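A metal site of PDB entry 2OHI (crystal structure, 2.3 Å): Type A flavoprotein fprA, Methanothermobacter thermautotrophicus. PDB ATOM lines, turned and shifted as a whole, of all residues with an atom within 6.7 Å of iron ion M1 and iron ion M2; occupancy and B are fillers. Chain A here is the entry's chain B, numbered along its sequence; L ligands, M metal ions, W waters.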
ATOM      1  N   TYR A  25     -13.995  12.421 -24.708  1.00  0.00           N
ATOM      2  CA  TYR A  25     -13.302  13.427 -23.919  1.00  0.00           C
ATOM      3  C   TYR A  25     -12.325  12.735 -22.964  1.00  0.00           C
ATOM      4  O   TYR A  25     -12.688  12.339 -21.853  1.00  0.00           O
ATOM      5  CB  TYR A  25     -14.288  14.344 -23.194  1.00  0.00           C
ATOM      6  CG  TYR A  25     -13.651  15.416 -22.351  1.00  0.00           C
ATOM      7  CD1 TYR A  25     -12.524  16.118 -22.803  1.00  0.00           C
ATOM      8  CD2 TYR A  25     -14.168  15.747 -21.084  1.00  0.00           C
ATOM      9  CE1 TYR A  25     -11.913  17.109 -22.034  1.00  0.00           C
ATOM     10  CE2 TYR A  25     -13.570  16.746 -20.288  1.00  0.00           C
ATOM     11  CZ  TYR A  25     -12.441  17.422 -20.774  1.00  0.00           C
ATOM     12  OH  TYR A  25     -11.831  18.405 -20.010  1.00  0.00           O
ATOM     13  N   HIS A  26     -11.085  12.605 -23.434  1.00  0.00           N
ATOM     14  CA  HIS A  26      -9.983  11.915 -22.729  1.00  0.00           C
ATOM     15  C   HIS A  26     -10.325  10.545 -22.118  1.00  0.00           C
ATOM     16  O   HIS A  26     -10.160  10.320 -20.907  1.00  0.00           O
ATOM     17  CB  HIS A  26      -9.233  12.861 -21.756  1.00  0.00           C
ATOM     18  CG  HIS A  26     -10.025  13.363 -20.588  1.00  0.00           C
ATOM     19  ND1 HIS A  26     -10.204  14.702 -20.341  1.00  0.00           N
ATOM     20  CD2 HIS A  26     -10.660  12.705 -19.586  1.00  0.00           C
ATOM     21  CE1 HIS A  26     -10.930  14.847 -19.232  1.00  0.00           C
ATOM     22  NE2 HIS A  26     -11.223  13.656 -18.762  1.00  0.00           N
ATOM     23  N   TYR A  35     -19.534  23.795 -22.346  1.00  0.00           N
ATOM     24  CA  TYR A  35     -18.635  24.438 -21.400  1.00  0.00           C
ATOM     25  C   TYR A  35     -19.378  25.633 -20.881  1.00  0.00           C
ATOM     26  O   TYR A  35     -19.664  26.576 -21.631  1.00  0.00           O
ATOM     27  CB  TYR A  35     -17.306  24.823 -22.042  1.00  0.00           C
ATOM     28  CG  TYR A  35     -16.770  23.711 -22.876  1.00  0.00           C
ATOM     29  CD1 TYR A  35     -16.310  22.534 -22.292  1.00  0.00           C
ATOM     30  CD2 TYR A  35     -16.768  23.794 -24.277  1.00  0.00           C
ATOM     31  CE1 TYR A  35     -15.853  21.477 -23.052  1.00  0.00           C
ATOM     32  CE2 TYR A  35     -16.302  22.738 -25.041  1.00  0.00           C
ATOM     33  CZ  TYR A  35     -15.852  21.594 -24.414  1.00  0.00           C
ATOM     34  OH  TYR A  35     -15.407  20.543 -25.148  1.00  0.00           O
ATOM     35  N   HIS A  83     -11.446  27.094 -11.878  1.00  0.00           N
ATOM     36  CA  HIS A  83     -10.686  25.901 -12.225  1.00  0.00           C
ATOM     37  C   HIS A  83      -9.762  26.160 -13.433  1.00  0.00           C
ATOM     38  O   HIS A  83     -10.106  26.943 -14.313  1.00  0.00           O
ATOM     39  CB  HIS A  83     -11.708  24.811 -12.529  1.00  0.00           C
ATOM     40  CG  HIS A  83     -11.120  23.452 -12.737  1.00  0.00           C
ATOM     41  ND1 HIS A  83      -9.888  23.084 -12.250  1.00  0.00           N
ATOM     42  CD2 HIS A  83     -11.633  22.355 -13.353  1.00  0.00           C
ATOM     43  CE1 HIS A  83      -9.649  21.823 -12.582  1.00  0.00           C
ATOM     44  NE2 HIS A  83     -10.701  21.359 -13.237  1.00  0.00           N
ATOM     45  N   GLU A  85      -8.310  23.750 -15.612  1.00  0.00           N
ATOM     46  CA  GLU A  85      -8.358  22.807 -16.726  1.00  0.00           C
ATOM     47  C   GLU A  85      -8.692  23.512 -18.057  1.00  0.00           C
ATOM     48  O   GLU A  85      -9.478  24.458 -18.088  1.00  0.00           O
ATOM     49  CB  GLU A  85      -9.309  21.647 -16.433  1.00  0.00           C
ATOM     50  CG  GLU A  85      -9.160  20.456 -17.378  1.00  0.00           C
ATOM     51  CD  GLU A  85      -9.948  19.221 -16.947  1.00  0.00           C
ATOM     52  OE1 GLU A  85      -9.772  18.802 -15.776  1.00  0.00           O
ATOM     53  OE2 GLU A  85     -10.728  18.666 -17.757  1.00  0.00           O
ATOM     54  N   ASP A  87     -10.544  23.135 -20.613  1.00  0.00           N
ATOM     55  CA  ASP A  87     -11.886  23.339 -21.147  1.00  0.00           C
ATOM     56  C   ASP A  87     -12.656  24.485 -20.484  1.00  0.00           C
ATOM     57  O   ASP A  87     -13.710  24.888 -20.978  1.00  0.00           O
ATOM     58  CB  ASP A  87     -12.724  22.055 -21.165  1.00  0.00           C
ATOM     59  CG  ASP A  87     -12.545  21.198 -19.928  1.00  0.00           C
ATOM     60  OD1 ASP A  87     -11.377  20.989 -19.519  1.00  0.00           O
ATOM     61  OD2 ASP A  87     -13.551  20.682 -19.392  1.00  0.00           O
ATOM     62  N   HIS A  88     -12.114  25.012 -19.390  1.00  0.00           N
ATOM     63  CA  HIS A  88     -12.725  26.122 -18.681  1.00  0.00           C
ATOM     64  C   HIS A  88     -11.848  27.379 -18.665  1.00  0.00           C
ATOM     65  O   HIS A  88     -12.305  28.428 -18.243  1.00  0.00           O
ATOM     66  CB  HIS A  88     -13.073  25.706 -17.262  1.00  0.00           C
ATOM     67  CG  HIS A  88     -13.830  24.415 -17.194  1.00  0.00           C
ATOM     68  ND1 HIS A  88     -15.089  24.274 -17.719  1.00  0.00           N
ATOM     69  CD2 HIS A  88     -13.486  23.208 -16.690  1.00  0.00           C
ATOM     70  CE1 HIS A  88     -15.505  23.035 -17.532  1.00  0.00           C
ATOM     71  NE2 HIS A  88     -14.552  22.366 -16.905  1.00  0.00           N
ATOM     72  N   HIS A 151     -12.536  19.077  -8.380  1.00  0.00           N
ATOM     73  CA  HIS A 151     -11.791  17.827  -8.555  1.00  0.00           C
ATOM     74  C   HIS A 151     -10.270  17.955  -8.716  1.00  0.00           C
ATOM     75  O   HIS A 151      -9.570  16.945  -8.862  1.00  0.00           O
ATOM     76  CB  HIS A 151     -12.434  16.959  -9.655  1.00  0.00           C
ATOM     77  CG  HIS A 151     -11.835  17.135 -11.013  1.00  0.00           C
ATOM     78  ND1 HIS A 151     -11.014  16.195 -11.592  1.00  0.00           N
ATOM     79  CD2 HIS A 151     -11.973  18.133 -11.932  1.00  0.00           C
ATOM     80  CE1 HIS A 151     -10.661  16.599 -12.802  1.00  0.00           C
ATOM     81  NE2 HIS A 151     -11.234  17.772 -13.032  1.00  0.00           N
ATOM     82  N   TRP A 152      -9.762  19.199  -8.662  1.00  0.00           N
ATOM     83  CA  TRP A 152      -8.315  19.494  -8.736  1.00  0.00           C
ATOM     84  C   TRP A 152      -7.835  20.381  -7.570  1.00  0.00           C
ATOM     85  O   TRP A 152      -8.623  21.139  -6.997  1.00  0.00           O
ATOM     86  CB  TRP A 152      -7.987  20.177 -10.080  1.00  0.00           C
ATOM     87  CG  TRP A 152      -7.770  19.267 -11.281  1.00  0.00           C
ATOM     88  CD1 TRP A 152      -8.098  17.936 -11.394  1.00  0.00           C
ATOM     89  CD2 TRP A 152      -7.215  19.633 -12.553  1.00  0.00           C
ATOM     90  NE1 TRP A 152      -7.767  17.474 -12.639  1.00  0.00           N
ATOM     91  CE2 TRP A 152      -7.229  18.490 -13.368  1.00  0.00           C
ATOM     92  CE3 TRP A 152      -6.693  20.837 -13.076  1.00  0.00           C
ATOM     93  CZ2 TRP A 152      -6.739  18.497 -14.696  1.00  0.00           C
ATOM     94  CZ3 TRP A 152      -6.216  20.835 -14.389  1.00  0.00           C
ATOM     95  CH2 TRP A 152      -6.240  19.678 -15.181  1.00  0.00           C
ATOM     96  N   ASN A 169     -18.086  24.633 -10.620  1.00  0.00           N
ATOM     97  CA  ASN A 169     -17.208  24.051 -11.651  1.00  0.00           C
ATOM     98  C   ASN A 169     -17.613  22.639 -12.058  1.00  0.00           C
ATOM     99  O   ASN A 169     -18.793  22.418 -12.357  1.00  0.00           O
ATOM    100  CB  ASN A 169     -15.721  24.170 -11.302  1.00  0.00           C
ATOM    101  CG  ASN A 169     -14.869  24.347 -12.558  1.00  0.00           C
ATOM    102  OD1 ASN A 169     -14.685  25.471 -13.057  1.00  0.00           O
ATOM    103  ND2 ASN A 169     -14.370  23.245 -13.087  1.00  0.00           N
ATOM    104  N   ASP A 170     -16.667  21.695 -12.089  1.00  0.00           N
ATOM    105  CA  ASP A 170     -16.938  20.327 -12.526  1.00  0.00           C
ATOM    106  C   ASP A 170     -17.988  19.633 -11.657  1.00  0.00           C
ATOM    107  O   ASP A 170     -18.830  18.919 -12.194  1.00  0.00           O
ATOM    108  CB  ASP A 170     -15.654  19.468 -12.606  1.00  0.00           C
ATOM    109  CG  ASP A 170     -14.761  19.837 -13.809  1.00  0.00           C
ATOM    110  OD1 ASP A 170     -15.251  19.880 -14.957  1.00  0.00           O
ATOM    111  OD2 ASP A 170     -13.539  20.056 -13.618  1.00  0.00           O
ATOM    112  N   HIS A 175     -22.017  15.498 -18.821  1.00  0.00           N
ATOM    113  CA  HIS A 175     -21.653  15.723 -20.215  1.00  0.00           C
ATOM    114  C   HIS A 175     -22.838  15.448 -21.119  1.00  0.00           C
ATOM    115  O   HIS A 175     -23.143  14.282 -21.438  1.00  0.00           O
ATOM    116  CB  HIS A 175     -20.436  14.896 -20.646  1.00  0.00           C
ATOM    117  CG  HIS A 175     -19.163  15.252 -19.939  1.00  0.00           C
ATOM    118  ND1 HIS A 175     -18.518  16.448 -20.153  1.00  0.00           N
ATOM    119  CD2 HIS A 175     -18.416  14.569 -19.051  1.00  0.00           C
ATOM    120  CE1 HIS A 175     -17.428  16.485 -19.401  1.00  0.00           C
ATOM    121  NE2 HIS A 175     -17.339  15.360 -18.730  1.00  0.00           N
ATOM    122  N   PHE A 198     -20.801  10.886 -14.701  1.00  0.00           N
ATOM    123  CA  PHE A 198     -19.817  11.910 -14.385  1.00  0.00           C
ATOM    124  C   PHE A 198     -19.236  11.556 -13.014  1.00  0.00           C
ATOM    125  O   PHE A 198     -18.021  11.590 -12.821  1.00  0.00           O
ATOM    126  CB  PHE A 198     -20.480  13.284 -14.398  1.00  0.00           C
ATOM    127  CG  PHE A 198     -19.506  14.439 -14.460  1.00  0.00           C
ATOM    128  CD1 PHE A 198     -19.225  15.058 -15.687  1.00  0.00           C
ATOM    129  CD2 PHE A 198     -18.907  14.937 -13.298  1.00  0.00           C
ATOM    130  CE1 PHE A 198     -18.362  16.146 -15.777  1.00  0.00           C
ATOM    131  CE2 PHE A 198     -18.024  16.024 -13.372  1.00  0.00           C
ATOM    132  CZ  PHE A 198     -17.745  16.631 -14.634  1.00  0.00           C
ATOM    133  N   LEU A 202     -15.302  10.527 -12.256  1.00  0.00           N
ATOM    134  CA  LEU A 202     -14.558  11.714 -11.857  1.00  0.00           C
ATOM    135  C   LEU A 202     -14.597  11.999 -10.348  1.00  0.00           C
ATOM    136  O   LEU A 202     -13.627  12.478  -9.774  1.00  0.00           O
ATOM    137  CB  LEU A 202     -15.043  12.929 -12.687  1.00  0.00           C
ATOM    138  CG  LEU A 202     -14.666  12.911 -14.189  1.00  0.00           C
ATOM    139  CD1 LEU A 202     -15.298  14.022 -14.971  1.00  0.00           C
ATOM    140  CD2 LEU A 202     -13.140  12.961 -14.397  1.00  0.00           C
ATOM    141  N   SER A 232     -20.070  23.582 -14.646  1.00  0.00           N
ATOM    142  CA  SER A 232     -19.390  23.989 -15.891  1.00  0.00           C
ATOM    143  C   SER A 232     -19.640  23.013 -17.051  1.00  0.00           C
ATOM    144  O   SER A 232     -19.163  23.224 -18.161  1.00  0.00           O
ATOM    145  CB  SER A 232     -17.910  24.110 -15.633  1.00  0.00           C
ATOM    146  OG  SER A 232     -17.397  22.838 -15.304  1.00  0.00           O
ATOM    147  N   HIS A 233     -20.361  21.921 -16.783  1.00  0.00           N
ATOM    148  CA  HIS A 233     -20.778  21.024 -17.856  1.00  0.00           C
ATOM    149  C   HIS A 233     -22.237  20.663 -17.686  1.00  0.00           C
ATOM    150  O   HIS A 233     -22.684  20.342 -16.581  1.00  0.00           O
ATOM    151  CB  HIS A 233     -19.974  19.726 -17.867  1.00  0.00           C
ATOM    152  CG  HIS A 233     -18.509  19.917 -18.128  1.00  0.00           C
ATOM    153  ND1 HIS A 233     -18.011  20.289 -19.349  1.00  0.00           N
ATOM    154  CD2 HIS A 233     -17.433  19.737 -17.326  1.00  0.00           C
ATOM    155  CE1 HIS A 233     -16.687  20.371 -19.292  1.00  0.00           C
ATOM    156  NE2 HIS A 233     -16.315  20.029 -18.067  1.00  0.00           N
HETATM  157  N1  LIG L   1      -2.352  15.086 -11.886  1.00  0.00           N
HETATM  158  C1  LIG L   1      -1.672  14.652 -10.785  1.00  0.00           C
HETATM  159  O1  LIG L   1      -0.519  15.008 -10.588  1.00  0.00           O
HETATM  160  N2  LIG L   1      -2.299  13.807  -9.902  1.00  0.00           N
HETATM  161  C2  LIG L   1      -3.584  13.376 -10.079  1.00  0.00           C
HETATM  162  O2  LIG L   1      -3.836  12.325  -9.499  1.00  0.00           O
HETATM  163  C3  LIG L   1      -4.283  13.803 -11.202  1.00  0.00           C
HETATM  164  N3  LIG L   1      -5.597  13.428 -11.472  1.00  0.00           N
HETATM  165  C4  LIG L   1      -6.234  13.889 -12.619  1.00  0.00           C
HETATM  166  C5  LIG L   1      -7.552  13.525 -12.920  1.00  0.00           C
HETATM  167  C6  LIG L   1      -8.213  13.979 -14.072  1.00  0.00           C
HETATM  168  C7  LIG L   1      -9.343  13.150 -14.612  1.00  0.00           C
HETATM  169  C8  LIG L   1      -7.550  14.827 -14.946  1.00  0.00           C
HETATM  170  C9  LIG L   1      -8.277  15.503 -16.072  1.00  0.00           C
HETATM  171  C10 LIG L   1      -6.231  15.205 -14.663  1.00  0.00           C
HETATM  172  C11 LIG L   1      -5.576  14.734 -13.506  1.00  0.00           C
HETATM  173  N4  LIG L   1      -4.267  15.115 -13.243  1.00  0.00           N
HETATM  174  C12 LIG L   1      -3.645  14.671 -12.102  1.00  0.00           C
HETATM  175  C13 LIG L   1      -3.611  16.213 -14.020  1.00  0.00           C
HETATM  176  C14 LIG L   1      -2.880  15.746 -15.264  1.00  0.00           C
HETATM  177  O3  LIG L   1      -1.841  14.853 -14.926  1.00  0.00           O
HETATM  178  C15 LIG L   1      -2.340  16.994 -15.958  1.00  0.00           C
HETATM  179  O4  LIG L   1      -3.413  17.854 -16.261  1.00  0.00           O
HETATM  180  C16 LIG L   1      -1.447  16.745 -17.187  1.00  0.00           C
HETATM  181  O5  LIG L   1      -0.924  17.986 -17.641  1.00  0.00           O
HETATM  182  C17 LIG L   1      -2.115  16.037 -18.373  1.00  0.00           C
HETATM  183  O6  LIG L   1      -1.137  15.821 -19.364  1.00  0.00           O
HETATM  184  P1  LIG L   1      -1.547  15.694 -20.893  1.00  0.00           P
HETATM  185  O7  LIG L   1      -1.690  17.099 -21.432  1.00  0.00           O
HETATM  186  O8  LIG L   1      -0.499  15.002 -21.705  1.00  0.00           O
HETATM  187  O9  LIG L   1      -2.831  14.931 -20.963  1.00  0.00           O
HETATM  188 FE    FE M   1     -14.574  20.334 -16.883  1.00  0.00          FE
HETATM  189 FE    FE M   2     -11.739  19.426 -14.610  1.00  0.00          FE
HETATM  190  O   HOH W   1     -14.418  17.914 -16.470  1.00  0.00           O
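NE2 of His 88 sits close to OD2 of Asp 87.
OG of Ser 232 sits close to NE2 of His 88.
OG of Ser 232 sits at hydrogen-bond distance from N of Asp 170 (3.5 Å).
The side-chain carboxylate (OD2) of Asp 170 sits close to the side-chain amide nitrogen (ND2) of Asn 169.
The side-chain carboxylate (OD2) of Asp 87 lies close to a ring nitrogen (NE2) of His 233.
The side-chain carboxylate (OE2) of Glu 85 lies within hydrogen-bond range of the side-chain hydroxyl (OH) of Tyr 25 (2.5 Å).
The side-chain carboxylate of Asp 87 lies within hydrogen-bond range of the side-chain hydroxyl of Tyr 25 (2.7 Å).
The nearest printed residue that does not touch iron ion M1 is Ser 232 (4.1 Å).
The nearest printed residue that does not touch iron ion M2 is His 88 (4.7 Å).
Iron ion M1 is bound by a ring nitrogen (NE2) of His 88 (2.0 Å), the side-chain carboxylate (OD1) of Asp 170 (2.1 Å), a ring nitrogen (NE2) of His 233 (2.1 Å) and water W1 (2.5 Å).
Iron ion M1 has four donor atoms within binding distance.
Slightly farther from iron ion M1 lies OD2 of Asp 87 (2.7 Å).
Iron ion M2 is bound by the side-chain carboxylate (OD2) of Asp 170 (2.1 Å), a ring nitrogen (NE2) of His 151 (2.3 Å), the side-chain carboxylate (OE1) of Glu 85 (2.4 Å) and a ring nitrogen (NE2) of His 83 (2.6 Å).
Iron ion M2 has four donor atoms within binding distance.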
